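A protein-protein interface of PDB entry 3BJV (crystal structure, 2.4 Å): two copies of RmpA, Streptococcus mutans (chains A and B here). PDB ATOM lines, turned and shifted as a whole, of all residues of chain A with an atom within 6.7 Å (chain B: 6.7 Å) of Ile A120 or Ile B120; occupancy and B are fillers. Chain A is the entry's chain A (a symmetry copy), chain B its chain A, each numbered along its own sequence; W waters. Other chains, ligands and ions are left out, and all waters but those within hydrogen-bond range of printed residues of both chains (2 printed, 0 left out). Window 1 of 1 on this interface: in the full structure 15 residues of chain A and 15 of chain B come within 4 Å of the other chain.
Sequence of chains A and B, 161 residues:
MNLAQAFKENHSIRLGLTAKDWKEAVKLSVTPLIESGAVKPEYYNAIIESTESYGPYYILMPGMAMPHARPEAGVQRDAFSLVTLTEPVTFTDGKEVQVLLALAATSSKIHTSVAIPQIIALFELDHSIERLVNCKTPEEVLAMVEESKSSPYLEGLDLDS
OE2 of Glu B124 sits close to OE2 of Glu A124 (2.5 Å).
The side-chain carboxylate (OE2) of Glu B124 sits at hydrogen-bond distance from the side-chain hydroxyl (OH) of Tyr A153 (2.7 Å).
The side-chain hydroxyl (OH) of Tyr B153 lies within hydrogen-bond range of the side-chain carboxylate (OE2) of Glu A124, at 2.7 Å.
The side-chain sulfur (SD) of Met B64 sits at hydrogen-bond distance from the backbone NH (N) of Leu B60, 3.7 Å away.
The side-chain hydroxyl of Ser B151 sits close to the backbone NH of Tyr B153.
SD of Met A64 sits at hydrogen-bond distance from N of Leu A60, 3.7 Å away.
The backbone NH (N) of Tyr A153 lies close to the side-chain hydroxyl (OG) of Ser A151 (3.4 Å).
Among the printed residues, pairs that only touch across the chains: Tyr A153 with Leu B60 (3.4 Å), Leu A60 with Tyr B153 (3.4 Å), Ile A120 with Ile B120 (3.9 Å), Tyr A153 with Ile B120 (3.99 Å) and Ile A120 with Tyr B153 (3.99 Å).
Printed residues of chain B within 4 Å of Ile A120: Ile B120 (3.9 Å) and Tyr B153 (3.99 Å).
Printed residues of chain B within 4 Å of Tyr A153: Leu B60 (3.4 Å), Ile B120 (3.99 Å) and Glu B124 (2.7 Å).
Printed residues of chain A within 4 Å of Ile B120: Ile A120 and Tyr A153.
Of the printed residues of chain A, Tyr B153 touches Leu A60 (3.4 Å), Ile A120 (3.99 Å) and Glu A124 (2.7 Å).
The nearest printed residue of chain A that does not touch Leu B60 is Pro A117 (4.4 Å).
Of the 18 printed residues of chain A, 4 touch a printed residue of chain B.
Hydrophobic or aromatic side chains of chain A within 4 Å of the printed part of chain B: Ile A120 and Tyr A153.
Of the 18 printed residues of chain B, 4 touch a printed residue of chain A.
Hydrophobic or aromatic side chains of chain B within 4 Å of the printed part of chain A: Ile B120 and Tyr B153.
Among the printed residues, 8 pairs touch across the chains.
Leu A60 touches Tyr B153, and with the chains exchanged Tyr A153 touches Leu B60.
Ile A120 touches Tyr B153, and with the chains exchanged Tyr A153 touches Ile B120.
Glu B124 touches its own counterpart, Glu A124.
Glu A124 touches Tyr B153, and with the chains exchanged Tyr A153 touches Glu B124.
Positions printed for both chains: 60, 61, 64, 66, 115, 116, 117, 118, 119, 120, 121, 122, 123, 124, 125, 148, 151 and 153.
Water W2 lies within hydrogen-bond range of O of Leu B60 (2.5 Å) and O of Tyr A153 (2.6 Å).
Water W1 bridges O of Leu A60 (2.5 Å) and O of Tyr B153 (2.6 Å).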
ATOM      1  N   LEU A  60     -14.857  -2.141  -2.657  1.00  0.00           N
ATOM      2  CA  LEU A  60     -14.207  -1.440  -3.780  1.00  0.00           C
ATOM      3  C   LEU A  60     -13.047  -0.533  -3.446  1.00  0.00           C
ATOM      4  O   LEU A  60     -12.073  -0.460  -4.199  1.00  0.00           O
ATOM      5  CB  LEU A  60     -15.200  -0.626  -4.610  1.00  0.00           C
ATOM      6  CG  LEU A  60     -15.927  -1.373  -5.732  1.00  0.00           C
ATOM      7  CD1 LEU A  60     -16.400  -0.348  -6.741  1.00  0.00           C
ATOM      8  CD2 LEU A  60     -15.132  -2.556  -6.394  1.00  0.00           C
ATOM      9  N   MET A  61     -13.179   0.170  -2.334  1.00  0.00           N
ATOM     10  CA  MET A  61     -12.146   1.048  -1.835  1.00  0.00           C
ATOM     11  C   MET A  61     -12.284   1.013  -0.334  1.00  0.00           C
ATOM     12  O   MET A  61     -13.337   0.631   0.158  1.00  0.00           O
ATOM     13  CB  MET A  61     -12.305   2.468  -2.400  1.00  0.00           C
ATOM     14  CG  MET A  61     -13.684   3.164  -2.245  1.00  0.00           C
ATOM     15  SD  MET A  61     -13.698   4.916  -2.895  1.00  0.00           S
ATOM     16  CE  MET A  61     -13.254   5.909  -1.443  1.00  0.00           C
ATOM     17  N   MET A  64     -15.646   1.439   2.328  1.00  0.00           N
ATOM     18  CA  MET A  64     -16.961   1.090   1.798  1.00  0.00           C
ATOM     19  C   MET A  64     -17.108  -0.383   1.284  1.00  0.00           C
ATOM     20  O   MET A  64     -16.124  -1.028   0.895  1.00  0.00           O
ATOM     21  CB  MET A  64     -17.403   2.124   0.744  1.00  0.00           C
ATOM     22  CG  MET A  64     -16.718   2.007  -0.626  1.00  0.00           C
ATOM     23  SD  MET A  64     -17.238   0.567  -1.645  1.00  0.00           S
ATOM     24  CE  MET A  64     -18.743   1.205  -2.382  1.00  0.00           C
ATOM     25  N   MET A  66     -20.044  -2.684  -1.226  1.00  0.00           N
ATOM     26  CA  MET A  66     -21.306  -2.834  -1.962  1.00  0.00           C
ATOM     27  C   MET A  66     -21.811  -4.280  -1.935  1.00  0.00           C
ATOM     28  O   MET A  66     -21.725  -4.979  -2.937  1.00  0.00           O
ATOM     29  CB  MET A  66     -21.197  -2.320  -3.408  1.00  0.00           C
ATOM     30  CG  MET A  66     -19.871  -2.523  -3.980  1.00  0.00           C
ATOM     31  SD  MET A  66     -19.812  -2.171  -5.731  1.00  0.00           S
ATOM     32  CE  MET A  66     -20.717  -3.629  -6.367  1.00  0.00           C
ATOM     33  N   ALA A 115     -25.123   0.113 -12.568  1.00  0.00           N
ATOM     34  CA  ALA A 115     -24.970   0.213 -11.108  1.00  0.00           C
ATOM     35  C   ALA A 115     -23.609   0.707 -10.603  1.00  0.00           C
ATOM     36  O   ALA A 115     -23.558   1.647  -9.787  1.00  0.00           O
ATOM     37  CB  ALA A 115     -25.240  -1.148 -10.486  1.00  0.00           C
ATOM     38  N   ILE A 116     -22.523   0.072 -11.066  1.00  0.00           N
ATOM     39  CA  ILE A 116     -21.145   0.393 -10.675  1.00  0.00           C
ATOM     40  C   ILE A 116     -20.664   1.784 -11.046  1.00  0.00           C
ATOM     41  O   ILE A 116     -20.114   2.447 -10.203  1.00  0.00           O
ATOM     42  CB  ILE A 116     -20.121  -0.704 -11.175  1.00  0.00           C
ATOM     43  CG1 ILE A 116     -20.063  -1.882 -10.201  1.00  0.00           C
ATOM     44  CG2 ILE A 116     -18.696  -0.121 -11.505  1.00  0.00           C
ATOM     45  CD1 ILE A 116     -19.704  -3.115 -10.954  1.00  0.00           C
ATOM     46  N   PRO A 117     -20.880   2.244 -12.300  1.00  0.00           N
ATOM     47  CA  PRO A 117     -20.580   3.639 -12.573  1.00  0.00           C
ATOM     48  C   PRO A 117     -21.249   4.654 -11.594  1.00  0.00           C
ATOM     49  O   PRO A 117     -20.649   5.679 -11.276  1.00  0.00           O
ATOM     50  CB  PRO A 117     -21.167   3.832 -13.966  1.00  0.00           C
ATOM     51  CG  PRO A 117     -21.346   2.524 -14.553  1.00  0.00           C
ATOM     52  CD  PRO A 117     -21.475   1.567 -13.481  1.00  0.00           C
ATOM     53  N   GLN A 118     -22.472   4.398 -11.135  1.00  0.00           N
ATOM     54  CA  GLN A 118     -23.169   5.357 -10.270  1.00  0.00           C
ATOM     55  C   GLN A 118     -22.621   5.309  -8.874  1.00  0.00           C
ATOM     56  O   GLN A 118     -22.547   6.326  -8.189  1.00  0.00           O
ATOM     57  CB  GLN A 118     -24.658   5.048 -10.207  1.00  0.00           C
ATOM     58  CG  GLN A 118     -25.445   5.538 -11.424  1.00  0.00           C
ATOM     59  CD  GLN A 118     -26.890   5.149 -11.333  1.00  0.00           C
ATOM     60  OE1 GLN A 118     -27.312   4.043 -11.766  1.00  0.00           O
ATOM     61  NE2 GLN A 118     -27.676   6.035 -10.771  1.00  0.00           N
ATOM     62  N   ILE A 119     -22.237   4.109  -8.452  1.00  0.00           N
ATOM     63  CA  ILE A 119     -21.650   3.904  -7.144  1.00  0.00           C
ATOM     64  C   ILE A 119     -20.266   4.574  -7.078  1.00  0.00           C
ATOM     65  O   ILE A 119     -19.966   5.272  -6.089  1.00  0.00           O
ATOM     66  CB  ILE A 119     -21.619   2.415  -6.783  1.00  0.00           C
ATOM     67  CG1 ILE A 119     -23.061   1.965  -6.490  1.00  0.00           C
ATOM     68  CG2 ILE A 119     -20.634   2.130  -5.613  1.00  0.00           C
ATOM     69  CD1 ILE A 119     -23.315   0.437  -6.596  1.00  0.00           C
ATOM     70  N   ILE A 120     -19.465   4.399  -8.134  1.00  0.00           N
ATOM     71  CA  ILE A 120     -18.148   4.979  -8.122  1.00  0.00           C
ATOM     72  C   ILE A 120     -18.146   6.526  -8.214  1.00  0.00           C
ATOM     73  O   ILE A 120     -17.379   7.183  -7.484  1.00  0.00           O
ATOM     74  CB  ILE A 120     -17.041   4.203  -8.980  1.00  0.00           C
ATOM     75  CG1 ILE A 120     -17.194   4.334 -10.459  1.00  0.00           C
ATOM     76  CG2 ILE A 120     -16.953   2.671  -8.626  1.00  0.00           C
ATOM     77  CD1 ILE A 120     -16.734   2.937 -11.118  1.00  0.00           C
ATOM     78  N   ALA A 121     -19.073   7.087  -8.999  1.00  0.00           N
ATOM     79  CA  ALA A 121     -19.344   8.552  -8.994  1.00  0.00           C
ATOM     80  C   ALA A 121     -19.583   9.131  -7.582  1.00  0.00           C
ATOM     81  O   ALA A 121     -18.997  10.135  -7.215  1.00  0.00           O
ATOM     82  CB  ALA A 121     -20.548   8.885  -9.904  1.00  0.00           C
ATOM     83  N   LEU A 122     -20.464   8.496  -6.812  1.00  0.00           N
ATOM     84  CA  LEU A 122     -20.749   8.913  -5.418  1.00  0.00           C
ATOM     85  C   LEU A 122     -19.479   8.934  -4.551  1.00  0.00           C
ATOM     86  O   LEU A 122     -19.151   9.976  -3.935  1.00  0.00           O
ATOM     87  CB  LEU A 122     -21.821   7.999  -4.816  1.00  0.00           C
ATOM     88  CG  LEU A 122     -22.254   8.272  -3.385  1.00  0.00           C
ATOM     89  CD1 LEU A 122     -22.830   9.712  -3.265  1.00  0.00           C
ATOM     90  CD2 LEU A 122     -23.337   7.215  -2.964  1.00  0.00           C
ATOM     91  N   PHE A 123     -18.743   7.808  -4.560  1.00  0.00           N
ATOM     92  CA  PHE A 123     -17.592   7.628  -3.731  1.00  0.00           C
ATOM     93  C   PHE A 123     -16.354   8.374  -4.192  1.00  0.00           C
ATOM     94  O   PHE A 123     -15.437   8.548  -3.424  1.00  0.00           O
ATOM     95  CB  PHE A 123     -17.324   6.147  -3.498  1.00  0.00           C
ATOM     96  CG  PHE A 123     -18.298   5.533  -2.559  1.00  0.00           C
ATOM     97  CD1 PHE A 123     -18.155   5.708  -1.173  1.00  0.00           C
ATOM     98  CD2 PHE A 123     -19.390   4.801  -3.043  1.00  0.00           C
ATOM     99  CE1 PHE A 123     -19.082   5.157  -0.299  1.00  0.00           C
ATOM    100  CE2 PHE A 123     -20.324   4.243  -2.172  1.00  0.00           C
ATOM    101  CZ  PHE A 123     -20.172   4.423  -0.790  1.00  0.00           C
ATOM    102  N   GLU A 124     -16.330   8.853  -5.424  1.00  0.00           N
ATOM    103  CA  GLU A 124     -15.219   9.729  -5.836  1.00  0.00           C
ATOM    104  C   GLU A 124     -15.388  11.235  -5.566  1.00  0.00           C
ATOM    105  O   GLU A 124     -14.552  12.033  -5.995  1.00  0.00           O
ATOM    106  CB  GLU A 124     -14.880   9.500  -7.301  1.00  0.00           C
ATOM    107  CG  GLU A 124     -14.299   8.091  -7.527  1.00  0.00           C
ATOM    108  CD  GLU A 124     -13.845   7.877  -8.936  1.00  0.00           C
ATOM    109  OE1 GLU A 124     -14.148   8.734  -9.824  1.00  0.00           O
ATOM    110  OE2 GLU A 124     -13.185   6.842  -9.145  1.00  0.00           O
ATOM    111  N   LEU A 125     -16.479  11.644  -4.927  1.00  0.00           N
ATOM    112  CA  LEU A 125     -16.590  13.023  -4.464  1.00  0.00           C
ATOM    113  C   LEU A 125     -15.496  13.240  -3.422  1.00  0.00           C
ATOM    114  O   LEU A 125     -15.001  12.263  -2.827  1.00  0.00           O
ATOM    115  CB  LEU A 125     -17.949  13.230  -3.822  1.00  0.00           C
ATOM    116  CG  LEU A 125     -19.065  13.187  -4.834  1.00  0.00           C
ATOM    117  CD1 LEU A 125     -20.431  13.248  -4.135  1.00  0.00           C
ATOM    118  CD2 LEU A 125     -18.877  14.295  -5.864  1.00  0.00           C
ATOM    119  N   SER A 148     -22.790  14.088  -7.700  1.00  0.00           N
ATOM    120  CA  SER A 148     -22.015  13.040  -8.360  1.00  0.00           C
ATOM    121  C   SER A 148     -22.303  13.005  -9.846  1.00  0.00           C
ATOM    122  O   SER A 148     -21.566  12.413 -10.617  1.00  0.00           O
ATOM    123  CB  SER A 148     -22.340  11.671  -7.759  1.00  0.00           C
ATOM    124  OG  SER A 148     -23.647  11.201  -8.133  1.00  0.00           O
ATOM    125  N   SER A 151     -19.832  13.435 -12.900  1.00  0.00           N
ATOM    126  CA  SER A 151     -18.821  12.412 -13.114  1.00  0.00           C
ATOM    127  C   SER A 151     -18.803  12.004 -14.598  1.00  0.00           C
ATOM    128  O   SER A 151     -19.851  11.914 -15.212  1.00  0.00           O
ATOM    129  CB  SER A 151     -19.183  11.204 -12.238  1.00  0.00           C
ATOM    130  OG  SER A 151     -18.265  10.125 -12.351  1.00  0.00           O
ATOM    131  N   TYR A 153     -18.144   8.981 -15.570  1.00  0.00           N
ATOM    132  CA  TYR A 153     -18.858   7.717 -15.493  1.00  0.00           C
ATOM    133  C   TYR A 153     -20.347   7.858 -15.796  1.00  0.00           C
ATOM    134  O   TYR A 153     -21.004   6.906 -16.272  1.00  0.00           O
ATOM    135  CB  TYR A 153     -18.610   7.043 -14.132  1.00  0.00           C
ATOM    136  CG  TYR A 153     -17.156   6.697 -13.960  1.00  0.00           C
ATOM    137  CD1 TYR A 153     -16.370   7.330 -12.996  1.00  0.00           C
ATOM    138  CD2 TYR A 153     -16.552   5.774 -14.798  1.00  0.00           C
ATOM    139  CE1 TYR A 153     -15.026   7.042 -12.867  1.00  0.00           C
ATOM    140  CE2 TYR A 153     -15.232   5.487 -14.698  1.00  0.00           C
ATOM    141  CZ  TYR A 153     -14.461   6.112 -13.721  1.00  0.00           C
ATOM    142  OH  TYR A 153     -13.121   5.766 -13.621  1.00  0.00           O
ATOM    143  N   LEU B  60     -17.367   1.968 -20.025  1.00  0.00           N
ATOM    144  CA  LEU B  60     -17.337   2.588 -18.688  1.00  0.00           C
ATOM    145  C   LEU B  60     -17.253   4.094 -18.631  1.00  0.00           C
ATOM    146  O   LEU B  60     -17.866   4.723 -17.764  1.00  0.00           O
ATOM    147  CB  LEU B  60     -16.209   2.034 -17.816  1.00  0.00           C
ATOM    148  CG  LEU B  60     -16.522   0.763 -17.021  1.00  0.00           C
ATOM    149  CD1 LEU B  60     -15.556   0.695 -15.857  1.00  0.00           C
ATOM    150  CD2 LEU B  60     -18.019   0.582 -16.580  1.00  0.00           C
ATOM    151  N   MET B  61     -16.471   4.654 -19.538  1.00  0.00           N
ATOM    152  CA  MET B  61     -16.315   6.085 -19.663  1.00  0.00           C
ATOM    153  C   MET B  61     -16.068   6.333 -21.130  1.00  0.00           C
ATOM    154  O   MET B  61     -15.688   5.407 -21.833  1.00  0.00           O
ATOM    155  CB  MET B  61     -15.162   6.596 -18.785  1.00  0.00           C
ATOM    156  CG  MET B  61     -13.774   5.916 -18.938  1.00  0.00           C
ATOM    157  SD  MET B  61     -12.452   6.703 -17.876  1.00  0.00           S
ATOM    158  CE  MET B  61     -11.734   7.966 -18.962  1.00  0.00           C
ATOM    159  N   MET B  64     -13.403   4.553 -24.011  1.00  0.00           N
ATOM    160  CA  MET B  64     -12.975   3.180 -23.760  1.00  0.00           C
ATOM    161  C   MET B  64     -14.129   2.126 -23.656  1.00  0.00           C
ATOM    162  O   MET B  64     -15.274   2.459 -23.318  1.00  0.00           O
ATOM    163  CB  MET B  64     -12.026   3.129 -22.546  1.00  0.00           C
ATOM    164  CG  MET B  64     -12.700   3.268 -21.173  1.00  0.00           C
ATOM    165  SD  MET B  64     -13.674   1.807 -20.624  1.00  0.00           S
ATOM    166  CE  MET B  64     -12.374   0.772 -19.952  1.00  0.00           C
ATOM    167  N   MET B  66     -14.560  -2.108 -22.205  1.00  0.00           N
ATOM    168  CA  MET B  66     -14.031  -3.382 -21.700  1.00  0.00           C
ATOM    169  C   MET B  66     -14.883  -4.571 -22.154  1.00  0.00           C
ATOM    170  O   MET B  66     -15.621  -5.138 -21.357  1.00  0.00           O
ATOM    171  CB  MET B  66     -13.872  -3.376 -20.170  1.00  0.00           C
ATOM    172  CG  MET B  66     -14.889  -2.573 -19.500  1.00  0.00           C
ATOM    173  SD  MET B  66     -14.869  -2.773 -17.725  1.00  0.00           S
ATOM    174  CE  MET B  66     -15.581  -4.454 -17.597  1.00  0.00           C
ATOM    175  N   ALA B 115     -10.803  -7.472 -11.279  1.00  0.00           N
ATOM    176  CA  ALA B 115     -10.624  -6.929 -12.634  1.00  0.00           C
ATOM    177  C   ALA B 115     -10.967  -5.446 -12.819  1.00  0.00           C
ATOM    178  O   ALA B 115     -10.142  -4.685 -13.359  1.00  0.00           O
ATOM    179  CB  ALA B 115     -11.470  -7.735 -13.608  1.00  0.00           C
ATOM    180  N   ILE B 116     -12.173  -5.044 -12.394  1.00  0.00           N
ATOM    181  CA  ILE B 116     -12.678  -3.671 -12.510  1.00  0.00           C
ATOM    182  C   ILE B 116     -11.900  -2.617 -11.743  1.00  0.00           C
ATOM    183  O   ILE B 116     -11.586  -1.604 -12.315  1.00  0.00           O
ATOM    184  CB  ILE B 116     -14.221  -3.581 -12.173  1.00  0.00           C
ATOM    185  CG1 ILE B 116     -15.069  -3.937 -13.397  1.00  0.00           C
ATOM    186  CG2 ILE B 116     -14.639  -2.207 -11.527  1.00  0.00           C
ATOM    187  CD1 ILE B 116     -16.361  -4.516 -12.937  1.00  0.00           C
ATOM    188  N   PRO B 117     -11.568  -2.852 -10.452  1.00  0.00           N
ATOM    189  CA  PRO B 117     -10.667  -1.916  -9.802  1.00  0.00           C
ATOM    190  C   PRO B 117      -9.337  -1.647 -10.573  1.00  0.00           C
ATOM    191  O   PRO B 117      -8.831  -0.527 -10.543  1.00  0.00           O
ATOM    192  CB  PRO B 117     -10.347  -2.628  -8.492  1.00  0.00           C
ATOM    193  CG  PRO B 117     -11.362  -3.635  -8.282  1.00  0.00           C
ATOM    194  CD  PRO B 117     -11.910  -3.995  -9.566  1.00  0.00           C
ATOM    195  N   GLN B 118      -8.761  -2.648 -11.235  1.00  0.00           N
ATOM    196  CA  GLN B 118      -7.474  -2.461 -11.914  1.00  0.00           C
ATOM    197  C   GLN B 118      -7.655  -1.699 -13.195  1.00  0.00           C
ATOM    198  O   GLN B 118      -6.799  -0.911 -13.588  1.00  0.00           O
ATOM    199  CB  GLN B 118      -6.835  -3.802 -12.245  1.00  0.00           C
ATOM    200  CG  GLN B 118      -6.138  -4.466 -11.056  1.00  0.00           C
ATOM    201  CD  GLN B 118      -5.585  -5.810 -11.428  1.00  0.00           C
ATOM    202  OE1 GLN B 118      -6.274  -6.861 -11.345  1.00  0.00           O
ATOM    203  NE2 GLN B 118      -4.343  -5.810 -11.847  1.00  0.00           N
ATOM    204  N   ILE B 119      -8.783  -1.946 -13.851  1.00  0.00           N
ATOM    205  CA  ILE B 119      -9.124  -1.261 -15.082  1.00  0.00           C
ATOM    206  C   ILE B 119      -9.396   0.227 -14.798  1.00  0.00           C
ATOM    207  O   ILE B 119      -8.888   1.097 -15.533  1.00  0.00           O
ATOM    208  CB  ILE B 119     -10.283  -1.963 -15.798  1.00  0.00           C
ATOM    209  CG1 ILE B 119      -9.754  -3.286 -16.379  1.00  0.00           C
ATOM    210  CG2 ILE B 119     -10.939  -1.040 -16.864  1.00  0.00           C
ATOM    211  CD1 ILE B 119     -10.837  -4.353 -16.693  1.00  0.00           C
ATOM    212  N   ILE B 120     -10.144   0.504 -13.725  1.00  0.00           N
ATOM    213  CA  ILE B 120     -10.456   1.877 -13.421  1.00  0.00           C
ATOM    214  C   ILE B 120      -9.235   2.703 -12.944  1.00  0.00           C
ATOM    215  O   ILE B 120      -9.068   3.859 -13.381  1.00  0.00           O
ATOM    216  CB  ILE B 120     -11.838   2.118 -12.649  1.00  0.00           C
ATOM    217  CG1 ILE B 120     -11.835   1.696 -11.218  1.00  0.00           C
ATOM    218  CG2 ILE B 120     -13.066   1.437 -13.362  1.00  0.00           C
ATOM    219  CD1 ILE B 120     -13.305   1.132 -10.876  1.00  0.00           C
ATOM    220  N   ALA B 121      -8.343   2.074 -12.171  1.00  0.00           N
ATOM    221  CA  ALA B 121      -7.014   2.663 -11.842  1.00  0.00           C
ATOM    222  C   ALA B 121      -6.229   3.145 -13.082  1.00  0.00           C
ATOM    223  O   ALA B 121      -5.726   4.255 -13.107  1.00  0.00           O
ATOM    224  CB  ALA B 121      -6.157   1.657 -11.041  1.00  0.00           C
ATOM    225  N   LEU B 122      -6.117   2.287 -14.095  1.00  0.00           N
ATOM    226  CA  LEU B 122      -5.436   2.638 -15.364  1.00  0.00           C
ATOM    227  C   LEU B 122      -6.056   3.879 -16.027  1.00  0.00           C
ATOM    228  O   LEU B 122      -5.338   4.868 -16.313  1.00  0.00           O
ATOM    229  CB  LEU B 122      -5.456   1.432 -16.310  1.00  0.00           C
ATOM    230  CG  LEU B 122      -4.798   1.596 -17.669  1.00  0.00           C
ATOM    231  CD1 LEU B 122      -3.295   1.957 -17.498  1.00  0.00           C
ATOM    232  CD2 LEU B 122      -4.949   0.259 -18.479  1.00  0.00           C
ATOM    233  N   PHE B 123      -7.389   3.847 -16.205  1.00  0.00           N
ATOM    234  CA  PHE B 123      -8.103   4.875 -16.896  1.00  0.00           C
ATOM    235  C   PHE B 123      -8.298   6.155 -16.107  1.00  0.00           C
ATOM    236  O   PHE B 123      -8.599   7.175 -16.681  1.00  0.00           O
ATOM    237  CB  PHE B 123      -9.412   4.335 -17.457  1.00  0.00           C
ATOM    238  CG  PHE B 123      -9.207   3.456 -18.638  1.00  0.00           C
ATOM    239  CD1 PHE B 123      -8.972   4.015 -19.905  1.00  0.00           C
ATOM    240  CD2 PHE B 123      -9.209   2.063 -18.499  1.00  0.00           C
ATOM    241  CE1 PHE B 123      -8.752   3.192 -21.002  1.00  0.00           C
ATOM    242  CE2 PHE B 123      -8.992   1.230 -19.595  1.00  0.00           C
ATOM    243  CZ  PHE B 123      -8.758   1.797 -20.856  1.00  0.00           C
ATOM    244  N   GLU B 124      -8.088   6.128 -14.802  1.00  0.00           N
ATOM    245  CA  GLU B 124      -8.097   7.391 -14.043  1.00  0.00           C
ATOM    246  C   GLU B 124      -6.762   8.151 -13.946  1.00  0.00           C
ATOM    247  O   GLU B 124      -6.674   9.146 -13.226  1.00  0.00           O
ATOM    248  CB  GLU B 124      -8.669   7.168 -12.652  1.00  0.00           C
ATOM    249  CG  GLU B 124     -10.165   6.803 -12.713  1.00  0.00           C
ATOM    250  CD  GLU B 124     -10.785   6.694 -11.357  1.00  0.00           C
ATOM    251  OE1 GLU B 124     -10.038   6.699 -10.329  1.00  0.00           O
ATOM    252  OE2 GLU B 124     -12.026   6.599 -11.330  1.00  0.00           O
ATOM    253  N   LEU B 125      -5.711   7.665 -14.597  1.00  0.00           N
ATOM    254  CA  LEU B 125      -4.485   8.448 -14.710  1.00  0.00           C
ATOM    255  C   LEU B 125      -4.822   9.702 -15.513  1.00  0.00           C
ATOM    256  O   LEU B 125      -5.816   9.710 -16.265  1.00  0.00           O
ATOM    257  CB  LEU B 125      -3.436   7.640 -15.449  1.00  0.00           C
ATOM    258  CG  LEU B 125      -2.944   6.472 -14.634  1.00  0.00           C
ATOM    259  CD1 LEU B 125      -2.000   5.592 -15.466  1.00  0.00           C
ATOM    260  CD2 LEU B 125      -2.304   6.971 -13.343  1.00  0.00           C
ATOM    261  N   SER B 148      -0.402   3.276 -12.139  1.00  0.00           N
ATOM    262  CA  SER B 148      -1.779   3.153 -11.670  1.00  0.00           C
ATOM    263  C   SER B 148      -1.830   2.531 -10.290  1.00  0.00           C
ATOM    264  O   SER B 148      -2.835   2.601  -9.604  1.00  0.00           O
ATOM    265  CB  SER B 148      -2.601   2.294 -12.632  1.00  0.00           C
ATOM    266  OG  SER B 148      -2.255   0.900 -12.559  1.00  0.00           O
ATOM    267  N   SER B 151      -3.338   3.972  -6.933  1.00  0.00           N
ATOM    268  CA  SER B 151      -4.776   4.163  -6.854  1.00  0.00           C
ATOM    269  C   SER B 151      -5.304   3.581  -5.530  1.00  0.00           C
ATOM    270  O   SER B 151      -4.838   2.542  -5.099  1.00  0.00           O
ATOM    271  CB  SER B 151      -5.413   3.432  -8.044  1.00  0.00           C
ATOM    272  OG  SER B 151      -6.829   3.543  -8.087  1.00  0.00           O
ATOM    273  N   TYR B 153      -8.229   2.205  -5.271  1.00  0.00           N
ATOM    274  CA  TYR B 153      -8.807   0.961  -5.755  1.00  0.00           C
ATOM    275  C   TYR B 153      -7.856  -0.225  -5.621  1.00  0.00           C
ATOM    276  O   TYR B 153      -8.290  -1.391  -5.488  1.00  0.00           O
ATOM    277  CB  TYR B 153      -9.315   1.131  -7.197  1.00  0.00           C
ATOM    278  CG  TYR B 153     -10.425   2.145  -7.261  1.00  0.00           C
ATOM    279  CD1 TYR B 153     -10.258   3.360  -7.925  1.00  0.00           C
ATOM    280  CD2 TYR B 153     -11.625   1.910  -6.610  1.00  0.00           C
ATOM    281  CE1 TYR B 153     -11.264   4.307  -7.948  1.00  0.00           C
ATOM    282  CE2 TYR B 153     -12.618   2.830  -6.608  1.00  0.00           C
ATOM    283  CZ  TYR B 153     -12.449   4.033  -7.288  1.00  0.00           C
ATOM    284  OH  TYR B 153     -13.501   4.937  -7.298  1.00  0.00           O
HETATM  285  O   HOH W   1     -10.542  -2.408  -4.732  1.00  0.00           O
HETATM  286  O   HOH W   2     -20.391   4.742 -17.543  1.00  0.00           O
